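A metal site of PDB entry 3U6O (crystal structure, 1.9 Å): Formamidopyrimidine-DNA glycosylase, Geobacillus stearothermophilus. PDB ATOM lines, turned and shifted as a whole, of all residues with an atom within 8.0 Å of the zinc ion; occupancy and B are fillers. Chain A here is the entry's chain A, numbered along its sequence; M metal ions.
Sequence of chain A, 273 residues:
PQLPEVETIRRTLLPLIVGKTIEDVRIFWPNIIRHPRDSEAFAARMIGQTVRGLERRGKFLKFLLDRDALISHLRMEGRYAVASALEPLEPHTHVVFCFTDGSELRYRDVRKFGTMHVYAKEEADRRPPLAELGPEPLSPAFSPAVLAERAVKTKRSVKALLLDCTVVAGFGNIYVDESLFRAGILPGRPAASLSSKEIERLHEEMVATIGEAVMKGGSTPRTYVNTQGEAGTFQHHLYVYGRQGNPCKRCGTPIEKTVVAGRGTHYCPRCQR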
ATOM      1  N   PHE A 181     -22.281  12.106  -3.256  1.00  0.00           N
ATOM      2  CA  PHE A 181     -21.243  11.186  -3.687  1.00  0.00           C
ATOM      3  C   PHE A 181     -21.615   9.747  -3.345  1.00  0.00           C
ATOM      4  O   PHE A 181     -21.505   8.840  -4.171  1.00  0.00           O
ATOM      5  CB  PHE A 181     -19.887  11.510  -3.076  1.00  0.00           C
ATOM      6  CG  PHE A 181     -18.860  10.427  -3.307  1.00  0.00           C
ATOM      7  CD1 PHE A 181     -18.111  10.398  -4.475  1.00  0.00           C
ATOM      8  CD2 PHE A 181     -18.688   9.407  -2.376  1.00  0.00           C
ATOM      9  CE1 PHE A 181     -17.184   9.387  -4.699  1.00  0.00           C
ATOM     10  CE2 PHE A 181     -17.768   8.394  -2.592  1.00  0.00           C
ATOM     11  CZ  PHE A 181     -17.017   8.375  -3.757  1.00  0.00           C
ATOM     12  N   TYR A 239     -15.265  11.670   1.624  1.00  0.00           N
ATOM     13  CA  TYR A 239     -15.036  11.189   0.265  1.00  0.00           C
ATOM     14  C   TYR A 239     -14.700  12.298  -0.715  1.00  0.00           C
ATOM     15  O   TYR A 239     -13.845  12.133  -1.583  1.00  0.00           O
ATOM     16  CB  TYR A 239     -16.268  10.442  -0.238  1.00  0.00           C
ATOM     17  CG  TYR A 239     -16.492   9.103   0.416  1.00  0.00           C
ATOM     18  CD1 TYR A 239     -17.512   8.922   1.352  1.00  0.00           C
ATOM     19  CD2 TYR A 239     -15.685   8.013   0.119  1.00  0.00           C
ATOM     20  CE1 TYR A 239     -17.708   7.702   1.963  1.00  0.00           C
ATOM     21  CE2 TYR A 239     -15.876   6.785   0.719  1.00  0.00           C
ATOM     22  CZ  TYR A 239     -16.901   6.640   1.646  1.00  0.00           C
ATOM     23  OH  TYR A 239     -17.092   5.412   2.246  1.00  0.00           O
ATOM     24  N   VAL A 240     -15.383  13.436  -0.595  1.00  0.00           N
ATOM     25  CA  VAL A 240     -15.209  14.491  -1.585  1.00  0.00           C
ATOM     26  C   VAL A 240     -15.023  15.872  -0.992  1.00  0.00           C
ATOM     27  O   VAL A 240     -14.283  16.691  -1.532  1.00  0.00           O
ATOM     28  CB  VAL A 240     -16.397  14.538  -2.585  1.00  0.00           C
ATOM     29  CG1 VAL A 240     -16.412  13.278  -3.460  1.00  0.00           C
ATOM     30  CG2 VAL A 240     -17.713  14.693  -1.853  1.00  0.00           C
ATOM     31  N   PRO A 247      -7.146  12.138  -5.234  1.00  0.00           N
ATOM     32  CA  PRO A 247      -7.827  10.995  -5.837  1.00  0.00           C
ATOM     33  C   PRO A 247      -9.064  10.560  -5.053  1.00  0.00           C
ATOM     34  O   PRO A 247      -9.072  10.527  -3.812  1.00  0.00           O
ATOM     35  CB  PRO A 247      -6.767   9.897  -5.821  1.00  0.00           C
ATOM     36  CG  PRO A 247      -5.781  10.316  -4.782  1.00  0.00           C
ATOM     37  CD  PRO A 247      -5.771  11.812  -4.806  1.00  0.00           C
ATOM     38  N   CYS A 248     -10.124  10.247  -5.789  1.00  0.00           N
ATOM     39  CA  CYS A 248     -11.312   9.653  -5.205  1.00  0.00           C
ATOM     40  C   CYS A 248     -10.925   8.385  -4.455  1.00  0.00           C
ATOM     41  O   CYS A 248     -10.124   7.583  -4.936  1.00  0.00           O
ATOM     42  CB  CYS A 248     -12.317   9.332  -6.306  1.00  0.00           C
ATOM     43  SG  CYS A 248     -13.778   8.454  -5.740  1.00  0.00           S
ATOM     44  N   LYS A 249     -11.490   8.206  -3.264  1.00  0.00           N
ATOM     45  CA  LYS A 249     -11.161   7.029  -2.449  1.00  0.00           C
ATOM     46  C   LYS A 249     -11.770   5.755  -3.005  1.00  0.00           C
ATOM     47  O   LYS A 249     -11.417   4.660  -2.589  1.00  0.00           O
ATOM     48  CB  LYS A 249     -11.602   7.245  -0.992  1.00  0.00           C
ATOM     49  CG  LYS A 249     -10.872   8.390  -0.315  1.00  0.00           C
ATOM     50  CD  LYS A 249     -11.233   8.514   1.166  1.00  0.00           C
ATOM     51  CE  LYS A 249     -10.491   9.672   1.801  1.00  0.00           C
ATOM     52  NZ  LYS A 249     -10.884   9.909   3.211  1.00  0.00           N
ATOM     53  N   ARG A 250     -12.684   5.897  -3.964  1.00  0.00           N
ATOM     54  CA  ARG A 250     -13.369   4.756  -4.544  1.00  0.00           C
ATOM     55  C   ARG A 250     -12.843   4.395  -5.944  1.00  0.00           C
ATOM     56  O   ARG A 250     -12.801   3.228  -6.302  1.00  0.00           O
ATOM     57  CB  ARG A 250     -14.885   4.991  -4.598  1.00  0.00           C
ATOM     58  CG  ARG A 250     -15.560   5.136  -3.236  1.00  0.00           C
ATOM     59  CD  ARG A 250     -16.240   3.837  -2.799  1.00  0.00           C
ATOM     60  NE  ARG A 250     -17.016   3.996  -1.569  1.00  0.00           N
ATOM     61  CZ  ARG A 250     -18.306   4.318  -1.545  1.00  0.00           C
ATOM     62  NH1 ARG A 250     -18.972   4.523  -2.675  1.00  0.00           N
ATOM     63  NH2 ARG A 250     -18.934   4.441  -0.380  1.00  0.00           N
ATOM     64  N   CYS A 251     -12.448   5.404  -6.714  1.00  0.00           N
ATOM     65  CA  CYS A 251     -12.004   5.166  -8.104  1.00  0.00           C
ATOM     66  C   CYS A 251     -10.670   5.797  -8.502  1.00  0.00           C
ATOM     67  O   CYS A 251     -10.153   5.529  -9.584  1.00  0.00           O
ATOM     68  CB  CYS A 251     -13.098   5.581  -9.093  1.00  0.00           C
ATOM     69  SG  CYS A 251     -13.192   7.369  -9.377  1.00  0.00           S
ATOM     70  N   GLY A 252     -10.133   6.656  -7.645  1.00  0.00           N
ATOM     71  CA  GLY A 252      -8.832   7.268  -7.913  1.00  0.00           C
ATOM     72  C   GLY A 252      -8.863   8.465  -8.850  1.00  0.00           C
ATOM     73  O   GLY A 252      -7.844   9.099  -9.095  1.00  0.00           O
ATOM     74  N   THR A 253     -10.036   8.766  -9.387  1.00  0.00           N
ATOM     75  CA  THR A 253     -10.197   9.948 -10.240  1.00  0.00           C
ATOM     76  C   THR A 253     -10.056  11.203  -9.388  1.00  0.00           C
ATOM     77  O   THR A 253     -10.589  11.254  -8.292  1.00  0.00           O
ATOM     78  CB  THR A 253     -11.580   9.964 -10.903  1.00  0.00           C
ATOM     79  OG1 THR A 253     -11.725   8.823 -11.745  1.00  0.00           O
ATOM     80  CG2 THR A 253     -11.781  11.237 -11.729  1.00  0.00           C
ATOM     81  N   PRO A 254      -9.341  12.218  -9.904  1.00  0.00           N
ATOM     82  CA  PRO A 254      -9.214  13.451  -9.111  1.00  0.00           C
ATOM     83  C   PRO A 254     -10.571  14.064  -8.802  1.00  0.00           C
ATOM     84  O   PRO A 254     -11.381  14.281  -9.703  1.00  0.00           O
ATOM     85  CB  PRO A 254      -8.405  14.372 -10.033  1.00  0.00           C
ATOM     86  CG  PRO A 254      -7.611  13.427 -10.901  1.00  0.00           C
ATOM     87  CD  PRO A 254      -8.534  12.268 -11.137  1.00  0.00           C
ATOM     88  N   ILE A 255     -10.801  14.340  -7.523  1.00  0.00           N
ATOM     89  CA  ILE A 255     -12.006  15.034  -7.095  1.00  0.00           C
ATOM     90  C   ILE A 255     -11.975  16.448  -7.659  1.00  0.00           C
ATOM     91  O   ILE A 255     -10.932  17.098  -7.713  1.00  0.00           O
ATOM     92  CB  ILE A 255     -12.135  15.063  -5.563  1.00  0.00           C
ATOM     93  CG1 ILE A 255     -12.212  13.629  -5.018  1.00  0.00           C
ATOM     94  CG2 ILE A 255     -13.343  15.890  -5.119  1.00  0.00           C
ATOM     95  CD1 ILE A 255     -13.283  12.769  -5.704  1.00  0.00           C
ATOM     96  N   TYR A 267     -17.132  16.831  -5.989  1.00  0.00           N
ATOM     97  CA  TYR A 267     -17.700  15.613  -6.535  1.00  0.00           C
ATOM     98  C   TYR A 267     -16.651  14.817  -7.297  1.00  0.00           C
ATOM     99  O   TYR A 267     -15.619  15.337  -7.711  1.00  0.00           O
ATOM    100  CB  TYR A 267     -18.866  15.963  -7.468  1.00  0.00           C
ATOM    101  CG  TYR A 267     -18.435  16.787  -8.665  1.00  0.00           C
ATOM    102  CD1 TYR A 267     -18.112  16.164  -9.861  1.00  0.00           C
ATOM    103  CD2 TYR A 267     -18.312  18.170  -8.585  1.00  0.00           C
ATOM    104  CE1 TYR A 267     -17.694  16.900 -10.953  1.00  0.00           C
ATOM    105  CE2 TYR A 267     -17.893  18.915  -9.674  1.00  0.00           C
ATOM    106  CZ  TYR A 267     -17.585  18.270 -10.862  1.00  0.00           C
ATOM    107  OH  TYR A 267     -17.168  18.996 -11.958  1.00  0.00           O
ATOM    108  N   CYS A 268     -16.931  13.534  -7.469  1.00  0.00           N
ATOM    109  CA  CYS A 268     -16.121  12.718  -8.346  1.00  0.00           C
ATOM    110  C   CYS A 268     -16.831  12.585  -9.682  1.00  0.00           C
ATOM    111  O   CYS A 268     -17.976  12.109  -9.735  1.00  0.00           O
ATOM    112  CB  CYS A 268     -15.869  11.337  -7.747  1.00  0.00           C
ATOM    113  SG  CYS A 268     -15.051  10.293  -8.922  1.00  0.00           S
ATOM    114  N   PRO A 269     -16.186  13.040 -10.772  1.00  0.00           N
ATOM    115  CA  PRO A 269     -16.876  13.016 -12.064  1.00  0.00           C
ATOM    116  C   PRO A 269     -17.047  11.606 -12.608  1.00  0.00           C
ATOM    117  O   PRO A 269     -17.727  11.419 -13.613  1.00  0.00           O
ATOM    118  CB  PRO A 269     -15.952  13.832 -12.961  1.00  0.00           C
ATOM    119  CG  PRO A 269     -14.598  13.626 -12.385  1.00  0.00           C
ATOM    120  CD  PRO A 269     -14.810  13.547 -10.886  1.00  0.00           C
ATOM    121  N   ARG A 270     -16.433  10.618 -11.967  1.00  0.00           N
ATOM    122  CA  ARG A 270     -16.593   9.236 -12.412  1.00  0.00           C
ATOM    123  C   ARG A 270     -17.662   8.493 -11.617  1.00  0.00           C
ATOM    124  O   ARG A 270     -18.522   7.834 -12.184  1.00  0.00           O
ATOM    125  CB  ARG A 270     -15.261   8.477 -12.352  1.00  0.00           C
ATOM    126  CG  ARG A 270     -15.373   7.053 -12.874  1.00  0.00           C
ATOM    127  CD  ARG A 270     -14.045   6.317 -12.880  1.00  0.00           C
ATOM    128  NE  ARG A 270     -14.231   4.967 -13.410  1.00  0.00           N
ATOM    129  CZ  ARG A 270     -13.238   4.126 -13.683  1.00  0.00           C
ATOM    130  NH1 ARG A 270     -13.530   2.919 -14.165  1.00  0.00           N
ATOM    131  NH2 ARG A 270     -11.978   4.480 -13.499  1.00  0.00           N
ATOM    132  N   CYS A 271     -17.601   8.613 -10.288  1.00  0.00           N
ATOM    133  CA  CYS A 271     -18.552   7.925  -9.413  1.00  0.00           C
ATOM    134  C   CYS A 271     -19.953   8.529  -9.464  1.00  0.00           C
ATOM    135  O   CYS A 271     -20.950   7.846  -9.237  1.00  0.00           O
ATOM    136  CB  CYS A 271     -18.057   7.925  -7.962  1.00  0.00           C
ATOM    137  SG  CYS A 271     -16.636   6.837  -7.624  1.00  0.00           S
ATOM    138  N   GLN A 272     -20.044   9.829  -9.754  1.00  0.00           N
ATOM    139  CA  GLN A 272     -21.335  10.506  -9.741  1.00  0.00           C
ATOM    140  C   GLN A 272     -21.809  10.824 -11.164  1.00  0.00           C
ATOM    141  O   GLN A 272     -21.017  11.260 -11.999  1.00  0.00           O
ATOM    142  CB  GLN A 272     -21.250  11.779  -8.895  1.00  0.00           C
ATOM    143  CG  GLN A 272     -20.892  11.487  -7.448  1.00  0.00           C
ATOM    144  CD  GLN A 272     -20.523  12.729  -6.665  1.00  0.00           C
ATOM    145  OE1 GLN A 272     -19.354  12.929  -6.313  1.00  0.00           O
ATOM    146  NE2 GLN A 272     -21.515  13.562  -6.366  1.00  0.00           N
HETATM  147 ZN    ZN M   1     -14.780   8.231  -7.865  1.00  0.00          ZN
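The side-chain sulfur (SG) of Cys 268 lies close to the backbone NH (N) of Arg 270 (3.4 Å).
N of Cys 268 lies within hydrogen-bond range of OE1 of Gln 272 (2.8 Å).
SG of Cys 251 lies close to OG1 of Thr 253, at 3.1 Å.
The backbone NH of Arg 250 sits close to the side-chain sulfur of Cys 248, at 3.3 Å.
N of Cys 248 sits at hydrogen-bond distance from O of Thr 253, at 2.7 Å.
Of the 18 residues printed, 4 come within 4 Å of the zinc ion.
SG of Cys 268 is bound to the zinc ion (2.3 Å).
The side-chain sulfur (SG) of Cys 271 is bound to the zinc ion, at 2.3 Å.
The zinc ion is bound by the side-chain sulfur (SG) of Cys 251 (2.4 Å).
The zinc ion is bound by SG of Cys 248, 2.4 Å away.
The zinc ion has four donor atoms within binding distance.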
